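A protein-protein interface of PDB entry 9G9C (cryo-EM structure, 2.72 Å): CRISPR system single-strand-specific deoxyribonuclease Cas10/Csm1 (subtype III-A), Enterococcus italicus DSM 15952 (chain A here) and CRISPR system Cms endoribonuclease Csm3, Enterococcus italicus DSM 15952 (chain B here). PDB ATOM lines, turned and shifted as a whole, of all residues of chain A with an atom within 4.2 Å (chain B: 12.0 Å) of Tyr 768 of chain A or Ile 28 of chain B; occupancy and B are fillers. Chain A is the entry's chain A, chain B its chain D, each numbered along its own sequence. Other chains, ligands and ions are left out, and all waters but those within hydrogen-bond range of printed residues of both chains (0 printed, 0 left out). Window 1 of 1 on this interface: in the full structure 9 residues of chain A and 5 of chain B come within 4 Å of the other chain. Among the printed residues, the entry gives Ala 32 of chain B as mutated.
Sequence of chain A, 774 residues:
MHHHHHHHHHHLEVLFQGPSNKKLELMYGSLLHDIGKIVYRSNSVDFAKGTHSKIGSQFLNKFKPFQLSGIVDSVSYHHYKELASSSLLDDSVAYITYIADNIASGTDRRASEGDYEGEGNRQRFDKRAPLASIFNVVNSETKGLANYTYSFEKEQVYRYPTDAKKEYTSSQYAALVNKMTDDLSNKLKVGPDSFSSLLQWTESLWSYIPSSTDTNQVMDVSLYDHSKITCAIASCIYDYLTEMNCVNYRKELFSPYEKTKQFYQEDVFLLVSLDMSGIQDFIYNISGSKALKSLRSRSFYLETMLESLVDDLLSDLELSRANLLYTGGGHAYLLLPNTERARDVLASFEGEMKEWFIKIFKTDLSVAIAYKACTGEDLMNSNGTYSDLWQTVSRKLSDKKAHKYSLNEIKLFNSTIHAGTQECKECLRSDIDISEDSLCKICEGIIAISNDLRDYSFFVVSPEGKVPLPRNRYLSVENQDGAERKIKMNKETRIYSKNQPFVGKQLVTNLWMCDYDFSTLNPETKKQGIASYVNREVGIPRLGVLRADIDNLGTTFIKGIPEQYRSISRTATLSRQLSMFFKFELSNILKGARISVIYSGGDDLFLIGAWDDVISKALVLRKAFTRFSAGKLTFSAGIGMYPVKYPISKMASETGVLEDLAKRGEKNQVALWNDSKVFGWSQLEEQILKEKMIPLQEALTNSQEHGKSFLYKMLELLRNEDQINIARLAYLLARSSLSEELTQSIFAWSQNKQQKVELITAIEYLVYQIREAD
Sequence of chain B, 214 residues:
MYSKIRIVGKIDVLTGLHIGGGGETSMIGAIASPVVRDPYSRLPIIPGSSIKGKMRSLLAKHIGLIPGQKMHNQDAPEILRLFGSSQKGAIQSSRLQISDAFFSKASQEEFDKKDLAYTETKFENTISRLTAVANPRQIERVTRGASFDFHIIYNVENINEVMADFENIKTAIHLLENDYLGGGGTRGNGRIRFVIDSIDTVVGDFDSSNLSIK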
ATOM      1  N   GLY A 539      -3.188   3.446   3.909  1.00  0.00           N
ATOM      2  CA  GLY A 539      -2.314   3.324   2.726  1.00  0.00           C
ATOM      3  C   GLY A 539      -1.452   4.560   2.613  1.00  0.00           C
ATOM      4  O   GLY A 539      -1.864   5.621   3.122  1.00  0.00           O
ATOM      5  N   ILE A 540      -0.271   4.432   2.012  1.00  0.00           N
ATOM      6  CA  ILE A 540       0.588   5.635   1.800  1.00  0.00           C
ATOM      7  C   ILE A 540      -0.159   6.548   0.816  1.00  0.00           C
ATOM      8  O   ILE A 540      -0.754   6.016  -0.146  1.00  0.00           O
ATOM      9  CB  ILE A 540       2.004   5.239   1.329  1.00  0.00           C
ATOM     10  CG1 ILE A 540       2.996   6.393   1.473  1.00  0.00           C
ATOM     11  CG2 ILE A 540       2.000   4.665  -0.088  1.00  0.00           C
ATOM     12  CD1 ILE A 540       4.441   5.992   1.244  1.00  0.00           C
ATOM     13  N   TRP A 611      -2.006   4.691  -6.144  1.00  0.00           N
ATOM     14  CA  TRP A 611      -1.033   3.619  -6.485  1.00  0.00           C
ATOM     15  C   TRP A 611      -1.623   2.207  -6.353  1.00  0.00           C
ATOM     16  O   TRP A 611      -1.338   1.386  -7.240  1.00  0.00           O
ATOM     17  CB  TRP A 611       0.204   3.783  -5.587  1.00  0.00           C
ATOM     18  CG  TRP A 611      -0.087   3.560  -4.128  1.00  0.00           C
ATOM     19  CD1 TRP A 611      -0.563   4.470  -3.231  1.00  0.00           C
ATOM     20  CD2 TRP A 611       0.063   2.321  -3.401  1.00  0.00           C
ATOM     21  NE1 TRP A 611      -0.722   3.888  -2.003  1.00  0.00           N
ATOM     22  CE2 TRP A 611      -0.347   2.572  -2.075  1.00  0.00           C
ATOM     23  CE3 TRP A 611       0.496   1.035  -3.742  1.00  0.00           C
ATOM     24  CZ2 TRP A 611      -0.331   1.584  -1.096  1.00  0.00           C
ATOM     25  CZ3 TRP A 611       0.510   0.059  -2.772  1.00  0.00           C
ATOM     26  CH2 TRP A 611       0.095   0.330  -1.471  1.00  0.00           C
ATOM     27  N   MET A 641       5.514   5.311  -8.281  1.00  0.00           N
ATOM     28  CA  MET A 641       4.764   5.887  -7.135  1.00  0.00           C
ATOM     29  C   MET A 641       5.311   7.293  -6.854  1.00  0.00           C
ATOM     30  O   MET A 641       6.543   7.418  -6.682  1.00  0.00           O
ATOM     31  CB  MET A 641       4.914   5.009  -5.888  1.00  0.00           C
ATOM     32  CG  MET A 641       3.598   4.651  -5.230  1.00  0.00           C
ATOM     33  SD  MET A 641       3.792   3.508  -3.849  1.00  0.00           S
ATOM     34  CE  MET A 641       4.948   4.462  -2.856  1.00  0.00           C
ATOM     35  N   TRP A 673       7.599   0.599  -9.712  1.00  0.00           N
ATOM     36  CA  TRP A 673       8.281   1.477  -8.722  1.00  0.00           C
ATOM     37  C   TRP A 673       9.746   1.746  -9.067  1.00  0.00           C
ATOM     38  O   TRP A 673      10.092   2.934  -9.220  1.00  0.00           O
ATOM     39  CB  TRP A 673       8.150   0.896  -7.309  1.00  0.00           C
ATOM     40  CG  TRP A 673       6.731   0.797  -6.819  1.00  0.00           C
ATOM     41  CD1 TRP A 673       5.663   1.539  -7.227  1.00  0.00           C
ATOM     42  CD2 TRP A 673       6.237  -0.094  -5.796  1.00  0.00           C
ATOM     43  NE1 TRP A 673       4.537   1.164  -6.543  1.00  0.00           N
ATOM     44  CE2 TRP A 673       4.858   0.170  -5.657  1.00  0.00           C
ATOM     45  CE3 TRP A 673       6.822  -1.080  -4.997  1.00  0.00           C
ATOM     46  CZ2 TRP A 673       4.060  -0.521  -4.749  1.00  0.00           C
ATOM     47  CZ3 TRP A 673       6.031  -1.760  -4.098  1.00  0.00           C
ATOM     48  CH2 TRP A 673       4.672  -1.482  -3.978  1.00  0.00           C
ATOM     49  N   TYR A 712       9.858  -4.375   9.076  1.00  0.00           N
ATOM     50  CA  TYR A 712      11.003  -3.504   8.703  1.00  0.00           C
ATOM     51  C   TYR A 712      12.294  -4.253   8.997  1.00  0.00           C
ATOM     52  O   TYR A 712      13.214  -4.228   8.160  1.00  0.00           O
ATOM     53  CB  TYR A 712      10.913  -2.173   9.450  1.00  0.00           C
ATOM     54  CG  TYR A 712      10.111  -1.093   8.740  1.00  0.00           C
ATOM     55  CD1 TYR A 712      10.716  -0.226   7.840  1.00  0.00           C
ATOM     56  CD2 TYR A 712       8.752  -0.937   8.974  1.00  0.00           C
ATOM     57  CE1 TYR A 712       9.993   0.760   7.194  1.00  0.00           C
ATOM     58  CE2 TYR A 712       8.017   0.046   8.338  1.00  0.00           C
ATOM     59  CZ  TYR A 712       8.641   0.899   7.447  1.00  0.00           C
ATOM     60  OH  TYR A 712       7.921   1.871   6.822  1.00  0.00           O
ATOM     61  N   ARG A 719      17.224  -6.787   2.336  1.00  0.00           N
ATOM     62  CA  ARG A 719      17.905  -5.746   1.525  1.00  0.00           C
ATOM     63  C   ARG A 719      19.431  -5.886   1.603  1.00  0.00           C
ATOM     64  O   ARG A 719      20.091  -5.696   0.564  1.00  0.00           O
ATOM     65  CB  ARG A 719      17.411  -4.368   1.974  1.00  0.00           C
ATOM     66  CG  ARG A 719      16.011  -4.088   1.450  1.00  0.00           C
ATOM     67  CD  ARG A 719      15.556  -2.720   1.901  1.00  0.00           C
ATOM     68  NE  ARG A 719      14.299  -2.323   1.260  1.00  0.00           N
ATOM     69  CZ  ARG A 719      13.714  -1.164   1.502  1.00  0.00           C
ATOM     70  NH1 ARG A 719      14.299  -0.291   2.300  1.00  0.00           N
ATOM     71  NH2 ARG A 719      12.546  -0.880   0.960  1.00  0.00           N
ATOM     72  N   GLU A 764       7.244  -4.526   0.963  1.00  0.00           N
ATOM     73  CA  GLU A 764       7.170  -3.064   0.722  1.00  0.00           C
ATOM     74  C   GLU A 764       5.732  -2.680   0.359  1.00  0.00           C
ATOM     75  O   GLU A 764       5.241  -1.675   0.905  1.00  0.00           O
ATOM     76  CB  GLU A 764       8.093  -2.673  -0.427  1.00  0.00           C
ATOM     77  CG  GLU A 764       9.533  -2.438   0.011  1.00  0.00           C
ATOM     78  CD  GLU A 764      10.489  -2.708  -1.131  1.00  0.00           C
ATOM     79  OE1 GLU A 764      10.000  -3.187  -2.171  1.00  0.00           O
ATOM     80  OE2 GLU A 764      11.696  -2.429  -0.998  1.00  0.00           O
ATOM     81  N   TYR A 765       5.071  -3.489  -0.471  1.00  0.00           N
ATOM     82  CA  TYR A 765       3.669  -3.196  -0.859  1.00  0.00           C
ATOM     83  C   TYR A 765       2.796  -3.241   0.377  1.00  0.00           C
ATOM     84  O   TYR A 765       1.921  -2.371   0.544  1.00  0.00           O
ATOM     85  CB  TYR A 765       3.197  -4.255  -1.856  1.00  0.00           C
ATOM     86  CG  TYR A 765       1.850  -3.983  -2.509  1.00  0.00           C
ATOM     87  CD1 TYR A 765       0.659  -4.325  -1.878  1.00  0.00           C
ATOM     88  CD2 TYR A 765       1.770  -3.414  -3.774  1.00  0.00           C
ATOM     89  CE1 TYR A 765      -0.568  -4.080  -2.471  1.00  0.00           C
ATOM     90  CE2 TYR A 765       0.550  -3.171  -4.380  1.00  0.00           C
ATOM     91  CZ  TYR A 765      -0.622  -3.504  -3.727  1.00  0.00           C
ATOM     92  OH  TYR A 765      -1.825  -3.265  -4.324  1.00  0.00           O
ATOM     93  N   LEU A 766       3.029  -4.235   1.235  1.00  0.00           N
ATOM     94  CA  LEU A 766       2.227  -4.361   2.478  1.00  0.00           C
ATOM     95  C   LEU A 766       2.473  -3.141   3.374  1.00  0.00           C
ATOM     96  O   LEU A 766       1.499  -2.614   3.933  1.00  0.00           O
ATOM     97  CB  LEU A 766       2.580  -5.660   3.195  1.00  0.00           C
ATOM     98  CG  LEU A 766       1.766  -5.969   4.453  1.00  0.00           C
ATOM     99  CD1 LEU A 766       0.285  -5.902   4.135  1.00  0.00           C
ATOM    100  CD2 LEU A 766       2.137  -7.339   4.981  1.00  0.00           C
ATOM    101  N   VAL A 767       3.732  -2.710   3.485  1.00  0.00           N
ATOM    102  CA  VAL A 767       4.060  -1.537   4.351  1.00  0.00           C
ATOM    103  C   VAL A 767       3.363  -0.292   3.774  1.00  0.00           C
ATOM    104  O   VAL A 767       2.786   0.486   4.560  1.00  0.00           O
ATOM    105  CB  VAL A 767       5.563  -1.286   4.579  1.00  0.00           C
ATOM    106  CG1 VAL A 767       5.769  -0.148   5.565  1.00  0.00           C
ATOM    107  CG2 VAL A 767       6.269  -2.531   5.102  1.00  0.00           C
ATOM    108  N   TYR A 768       3.380  -0.141   2.447  1.00  0.00           N
ATOM    109  CA  TYR A 768       2.689   1.018   1.834  1.00  0.00           C
ATOM    110  C   TYR A 768       1.200   0.926   2.125  1.00  0.00           C
ATOM    111  O   TYR A 768       0.592   1.953   2.463  1.00  0.00           O
ATOM    112  CB  TYR A 768       2.948   0.973   0.328  1.00  0.00           C
ATOM    113  CG  TYR A 768       4.349   1.367  -0.116  1.00  0.00           C
ATOM    114  CD1 TYR A 768       5.019   2.423   0.482  1.00  0.00           C
ATOM    115  CD2 TYR A 768       5.004   0.668  -1.122  1.00  0.00           C
ATOM    116  CE1 TYR A 768       6.293   2.786   0.082  1.00  0.00           C
ATOM    117  CE2 TYR A 768       6.285   1.010  -1.521  1.00  0.00           C
ATOM    118  CZ  TYR A 768       6.930   2.074  -0.917  1.00  0.00           C
ATOM    119  OH  TYR A 768       8.187   2.433  -1.304  1.00  0.00           O
ATOM    120  N   GLN A 769       0.637  -0.279   2.047  1.00  0.00           N
ATOM    121  CA  GLN A 769      -0.811  -0.491   2.303  1.00  0.00           C
ATOM    122  C   GLN A 769      -1.135  -0.277   3.790  1.00  0.00           C
ATOM    123  O   GLN A 769      -2.098   0.456   4.087  1.00  0.00           O
ATOM    124  CB  GLN A 769      -1.135  -1.915   1.867  1.00  0.00           C
ATOM    125  CG  GLN A 769      -2.522  -2.403   2.262  1.00  0.00           C
ATOM    126  CD  GLN A 769      -2.574  -3.899   2.466  1.00  0.00           C
ATOM    127  OE1 GLN A 769      -2.924  -4.390   3.545  1.00  0.00           O
ATOM    128  NE2 GLN A 769      -2.216  -4.642   1.429  1.00  0.00           N
ATOM    129  N   ILE A 770      -0.380  -0.917   4.685  1.00  0.00           N
ATOM    130  CA  ILE A 770      -0.617  -0.784   6.159  1.00  0.00           C
ATOM    131  C   ILE A 770      -0.384   0.670   6.605  1.00  0.00           C
ATOM    132  O   ILE A 770      -1.151   1.134   7.474  1.00  0.00           O
ATOM    133  CB  ILE A 770       0.185  -1.808   6.991  1.00  0.00           C
ATOM    134  CG1 ILE A 770       1.693  -1.583   6.924  1.00  0.00           C
ATOM    135  CG2 ILE A 770      -0.194  -3.238   6.603  1.00  0.00           C
ATOM    136  CD1 ILE A 770       2.508  -2.730   7.491  1.00  0.00           C
ATOM    137  N   ARG A 771       0.611   1.366   6.041  1.00  0.00           N
ATOM    138  CA  ARG A 771       0.966   2.717   6.551  1.00  0.00           C
ATOM    139  C   ARG A 771      -0.223   3.670   6.423  1.00  0.00           C
ATOM    140  O   ARG A 771      -0.920   3.613   5.410  1.00  0.00           O
ATOM    141  CB  ARG A 771       2.115   3.289   5.716  1.00  0.00           C
ATOM    142  CG  ARG A 771       2.658   4.660   6.092  1.00  0.00           C
ATOM    143  CD  ARG A 771       3.951   4.944   5.346  1.00  0.00           C
ATOM    144  NE  ARG A 771       4.446   6.306   5.567  1.00  0.00           N
ATOM    145  CZ  ARG A 771       5.555   6.802   5.032  1.00  0.00           C
ATOM    146  NH1 ARG A 771       6.419   6.000   4.439  1.00  0.00           N
ATOM    147  NH2 ARG A 771       5.798   8.099   5.099  1.00  0.00           N
ATOM    148  N   SER B  26      12.755   7.142  -1.553  1.00  0.00           N
ATOM    149  CA  SER B  26      12.267   6.243  -2.632  1.00  0.00           C
ATOM    150  C   SER B  26      11.560   5.027  -2.016  1.00  0.00           C
ATOM    151  O   SER B  26      10.357   5.140  -1.696  1.00  0.00           O
ATOM    152  CB  SER B  26      13.399   5.819  -3.531  1.00  0.00           C
ATOM    153  OG  SER B  26      14.421   5.171  -2.787  1.00  0.00           O
ATOM    154  N   MET B  27      12.276   3.910  -1.877  1.00  0.00           N
ATOM    155  CA  MET B  27      11.702   2.699  -1.230  1.00  0.00           C
ATOM    156  C   MET B  27      11.509   2.950   0.275  1.00  0.00           C
ATOM    157  O   MET B  27      12.264   3.760   0.844  1.00  0.00           O
ATOM    158  CB  MET B  27      12.579   1.470  -1.480  1.00  0.00           C
ATOM    159  CG  MET B  27      12.190   0.707  -2.729  1.00  0.00           C
ATOM    160  SD  MET B  27      10.406   0.463  -2.857  1.00  0.00           S
ATOM    161  CE  MET B  27       9.977   1.566  -4.210  1.00  0.00           C
ATOM    162  N   ILE B  28      10.506   2.313   0.877  1.00  0.00           N
ATOM    163  CA  ILE B  28      10.207   2.517   2.327  1.00  0.00           C
ATOM    164  C   ILE B  28      11.374   1.956   3.160  1.00  0.00           C
ATOM    165  O   ILE B  28      12.008   0.988   2.703  1.00  0.00           O
ATOM    166  CB  ILE B  28       8.839   1.902   2.686  1.00  0.00           C
ATOM    167  CG1 ILE B  28       8.099   2.758   3.707  1.00  0.00           C
ATOM    168  CG2 ILE B  28       8.964   0.447   3.143  1.00  0.00           C
ATOM    169  CD1 ILE B  28       6.590   2.636   3.642  1.00  0.00           C
ATOM    170  N   GLY B  29      11.679   2.568   4.311  1.00  0.00           N
ATOM    171  CA  GLY B  29      12.812   2.124   5.150  1.00  0.00           C
ATOM    172  C   GLY B  29      14.118   2.199   4.393  1.00  0.00           C
ATOM    173  O   GLY B  29      14.969   1.312   4.596  1.00  0.00           O
ATOM    174  N   ALA B  30      14.279   3.223   3.561  1.00  0.00           N
ATOM    175  CA  ALA B  30      15.496   3.424   2.743  1.00  0.00           C
ATOM    176  C   ALA B  30      15.864   4.899   2.870  1.00  0.00           C
ATOM    177  O   ALA B  30      14.994   5.679   3.319  1.00  0.00           O
ATOM    178  CB  ALA B  30      15.256   3.017   1.315  1.00  0.00           C
ATOM    179  N   ILE B  31      17.094   5.288   2.517  1.00  0.00           N
ATOM    180  CA  ILE B  31      17.463   6.707   2.778  1.00  0.00           C
ATOM    181  C   ILE B  31      16.424   7.556   2.042  1.00  0.00           C
ATOM    182  O   ILE B  31      16.156   7.277   0.856  1.00  0.00           O
ATOM    183  CB  ILE B  31      18.879   7.008   2.254  1.00  0.00           C
ATOM    184  CG1 ILE B  31      19.797   5.796   2.365  1.00  0.00           C
ATOM    185  CG2 ILE B  31      19.479   8.228   2.947  1.00  0.00           C
ATOM    186  CD1 ILE B  31      21.153   6.002   1.716  1.00  0.00           C
ATOM    187  N   ALA B  32      15.898   8.577   2.715  1.00  0.00           N
ATOM    188  CA  ALA B  32      14.807   9.382   2.127  1.00  0.00           C
ATOM    189  C   ALA B  32      15.424  10.523   1.330  1.00  0.00           C
ATOM    190  O   ALA B  32      14.819  10.955   0.326  1.00  0.00           O
ATOM    191  CB  ALA B  32      13.904   9.882   3.228  1.00  0.00           C
ATOM    192  N   SER B  33      16.593  10.995   1.765  1.00  0.00           N
ATOM    193  CA  SER B  33      17.284  12.025   0.952  1.00  0.00           C
ATOM    194  C   SER B  33      18.631  11.493   0.466  1.00  0.00           C
ATOM    195  O   SER B  33      19.443  11.077   1.312  1.00  0.00           O
ATOM    196  CB  SER B  33      17.473  13.272   1.763  1.00  0.00           C
ATOM    197  OG  SER B  33      16.245  13.690   2.342  1.00  0.00           O
ATOM    198  N   THR B 121      24.974   7.124   5.648  1.00  0.00           N
ATOM    199  CA  THR B 121      23.574   7.463   5.976  1.00  0.00           C
ATOM    200  C   THR B 121      23.519   8.007   7.383  1.00  0.00           C
ATOM    201  O   THR B 121      24.179   7.426   8.266  1.00  0.00           O
ATOM    202  CB  THR B 121      22.682   6.234   5.827  1.00  0.00           C
ATOM    203  OG1 THR B 121      22.920   5.780   4.500  1.00  0.00           O
ATOM    204  CG2 THR B 121      21.210   6.557   6.012  1.00  0.00           C
ATOM    205  N   PHE B 123      20.939   9.008  10.586  1.00  0.00           N
ATOM    206  CA  PHE B 123      19.557   8.748  11.068  1.00  0.00           C
ATOM    207  C   PHE B 123      19.130   9.876  11.982  1.00  0.00           C
ATOM    208  O   PHE B 123      19.748  10.062  13.046  1.00  0.00           O
ATOM    209  CB  PHE B 123      19.538   7.377  11.746  1.00  0.00           C
ATOM    210  CG  PHE B 123      19.426   6.226  10.758  1.00  0.00           C
ATOM    211  CD1 PHE B 123      20.505   5.861   9.964  1.00  0.00           C
ATOM    212  CD2 PHE B 123      18.243   5.508  10.636  1.00  0.00           C
ATOM    213  CE1 PHE B 123      20.397   4.819   9.061  1.00  0.00           C
ATOM    214  CE2 PHE B 123      18.145   4.458   9.740  1.00  0.00           C
ATOM    215  CZ  PHE B 123      19.219   4.120   8.953  1.00  0.00           C
ATOM    216  N   ASN B 135       9.429  11.305  14.394  1.00  0.00           N
ATOM    217  CA  ASN B 135       9.231  10.888  12.980  1.00  0.00           C
ATOM    218  C   ASN B 135      10.601  10.693  12.337  1.00  0.00           C
ATOM    219  O   ASN B 135      11.279  11.707  12.079  1.00  0.00           O
ATOM    220  CB  ASN B 135       8.436  11.910  12.182  1.00  0.00           C
ATOM    221  CG  ASN B 135       8.309  11.521  10.728  1.00  0.00           C
ATOM    222  OD1 ASN B 135       8.717  12.282   9.846  1.00  0.00           O
ATOM    223  ND2 ASN B 135       7.742  10.354  10.459  1.00  0.00           N
ATOM    224  N   PRO B 136      11.033   9.449  12.046  1.00  0.00           N
ATOM    225  CA  PRO B 136      12.375   9.228  11.524  1.00  0.00           C
ATOM    226  C   PRO B 136      12.678   9.665  10.096  1.00  0.00           C
ATOM    227  O   PRO B 136      11.811   9.504   9.222  1.00  0.00           O
ATOM    228  CB  PRO B 136      12.534   7.702  11.673  1.00  0.00           C
ATOM    229  CG  PRO B 136      11.129   7.156  11.667  1.00  0.00           C
ATOM    230  CD  PRO B 136      10.254   8.247  12.240  1.00  0.00           C
ATOM    231  N   ARG B 137      13.872  10.217   9.866  1.00  0.00           N
ATOM    232  CA  ARG B 137      14.316  10.554   8.495  1.00  0.00           C
ATOM    233  C   ARG B 137      15.730   9.998   8.310  1.00  0.00           C
ATOM    234  O   ARG B 137      16.514  10.044   9.277  1.00  0.00           O
ATOM    235  CB  ARG B 137      14.319  12.067   8.261  1.00  0.00           C
ATOM    236  CG  ARG B 137      15.038  12.941   9.276  1.00  0.00           C
ATOM    237  CD  ARG B 137      15.123  14.365   8.759  1.00  0.00           C
ATOM    238  NE  ARG B 137      15.786  15.307   9.666  1.00  0.00           N
ATOM    239  CZ  ARG B 137      15.343  15.677  10.858  1.00  0.00           C
ATOM    240  NH1 ARG B 137      14.128  15.346  11.253  1.00  0.00           N
ATOM    241  NH2 ARG B 137      16.116  16.397  11.648  1.00  0.00           N
ATOM    242  N   GLN B 138      16.050   9.479   7.126  1.00  0.00           N
ATOM    243  CA  GLN B 138      17.442   9.035   6.871  1.00  0.00           C
ATOM    244  C   GLN B 138      18.024   9.918   5.759  1.00  0.00           C
ATOM    245  O   GLN B 138      17.375  10.037   4.704  1.00  0.00           O
ATOM    246  CB  GLN B 138      17.515   7.565   6.466  1.00  0.00           C
ATOM    247  CG  GLN B 138      16.474   6.674   7.133  1.00  0.00           C
ATOM    248  CD  GLN B 138      16.582   5.229   6.704  1.00  0.00           C
ATOM    249  OE1 GLN B 138      17.492   4.843   5.961  1.00  0.00           O
ATOM    250  NE2 GLN B 138      15.659   4.409   7.183  1.00  0.00           N
ATOM    251  N   ILE B 139      19.182  10.535   6.006  1.00  0.00           N
ATOM    252  CA  ILE B 139      19.815  11.432   4.992  1.00  0.00           C
ATOM    253  C   ILE B 139      21.187  10.854   4.632  1.00  0.00           C
ATOM    254  O   ILE B 139      21.754  10.122   5.454  1.00  0.00           O
ATOM    255  CB  ILE B 139      19.924  12.885   5.492  1.00  0.00           C
ATOM    256  CG1 ILE B 139      21.042  13.057   6.516  1.00  0.00           C
ATOM    257  CG2 ILE B 139      18.578  13.385   6.023  1.00  0.00           C
ATOM    258  CD1 ILE B 139      21.410  14.504   6.791  1.00  0.00           C
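OH of Tyr 768 of chain A sits at hydrogen-bond distance from SD of Met 27 of chain B (3.3 Å).
The side-chain hydroxyl (OH) of Tyr 768 of chain A sits at hydrogen-bond distance from the backbone NH (N) of Ile 28 of chain B (3.2 Å).
The side-chain carboxylate (OE2) of Glu 764 of chain A lies close to the side-chain sulfur (SD) of Met 27 of chain B (3.7 Å).
The guanidinium group (NH2) of Arg 719 of chain A sits at hydrogen-bond distance from the backbone carbonyl oxygen (O) of Ile 28 of chain B (2.6 Å).
O of Gly 29 of chain B sits at hydrogen-bond distance from NH1 of Arg 719 of chain A (2.9 Å).
OH of Tyr 768 of chain A lies within hydrogen-bond range of O of Ser 26 of chain B (3.5 Å).
The side-chain sulfur of Met 641 of chain A sits at hydrogen-bond distance from the indole nitrogen of Trp 673 of chain A, at 3.6 Å.
N of Ile 540 of chain A lies within hydrogen-bond range of O of Tyr 768 of chain A, at 2.7 Å.
NH2 of Arg 719 of chain A lies within salt-bridge range of OE2 of Glu 764 of chain A.
O of Arg 771 of chain A sits at hydrogen-bond distance from N of Gly 539 of chain A (2.7 Å).
Among the printed residues, merely in contact across the chains: Tyr 712 of chain A with Ile 28 of chain B (3.2 Å), Arg 719 of chain A with Met 27 of chain B (3.4 Å), Arg 771 of chain A with Ile 28 of chain B (3.5 Å), Val 767 of chain A with Ile 28 of chain B (3.5 Å), Arg 719 of chain A with Ala 30 of chain B (3.6 Å), Trp 673 of chain A with Met 27 of chain B (3.7 Å) and Tyr 712 of chain A with Gly 29 of chain B (3.7 Å).
Of chain B, only Ser 26, Met 27 and Ile 28 come within 4 Å of Tyr 768 of chain A.
Of chain A, only Tyr 712, Arg 719, Val 767, Tyr 768 and Arg 771 come within 4 Å of Ile 28 of chain B.
No residue of chain B comes within 4 Å of Gly 539 of chain A.
Glu 764 of chain A touches just one residue of chain B: Met 27 (3.6 Å).
No residue of chain B comes within 4 Å of Leu 766 of chain A.
Val 767 of chain A touches just one residue of chain B: Ile 28.
No residue of chain B comes within 4 Å of Ile 770 of chain A.
Of the printed residues of chain B, Arg 771 of chain A touches Ile 28.
Of the printed residues of chain A, Met 27 of chain B touches Trp 673, Arg 719, Glu 764 and Tyr 768.
Printed residues of chain B within 4 Å of Arg 719 of chain A: Met 27, Ile 28, Gly 29 and Ala 30.
Of the printed residues of chain A, Ser 26 of chain B touches Tyr 768 (3.5 Å).
Of the printed residues of chain A, Gly 29 of chain B touches Tyr 712 and Arg 719.
Of the printed residues of chain A, Ala 30 of chain B touches Arg 719 (3.6 Å).
Ala 32 of chain B touches none of the printed residues of chain A.
Asn 135 of chain B touches none of the printed residues of chain A.
Of the 15 printed residues of chain B, 5 touch a printed residue of chain A.
Printed residues of chain B that touch a printed residue of chain A: Ser 26, Met 27, Ile 28, Gly 29 and Ala 30.
Hydrophobic or aromatic side chains of chain B that line the printed part of chain A: Met 27, Ile 28 and Ala 30.
Of the 15 printed residues of chain A, 7 touch a printed residue of chain B.
Hydrophobic or aromatic side chains of chain A within 4 Å of the printed part of chain B: Trp 673, Tyr 712, Val 767 and Tyr 768.
Among the printed residues, no Asp or Glu carboxylate lies within 4 Å of a Lys or Arg side-chain nitrogen of the other chain.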
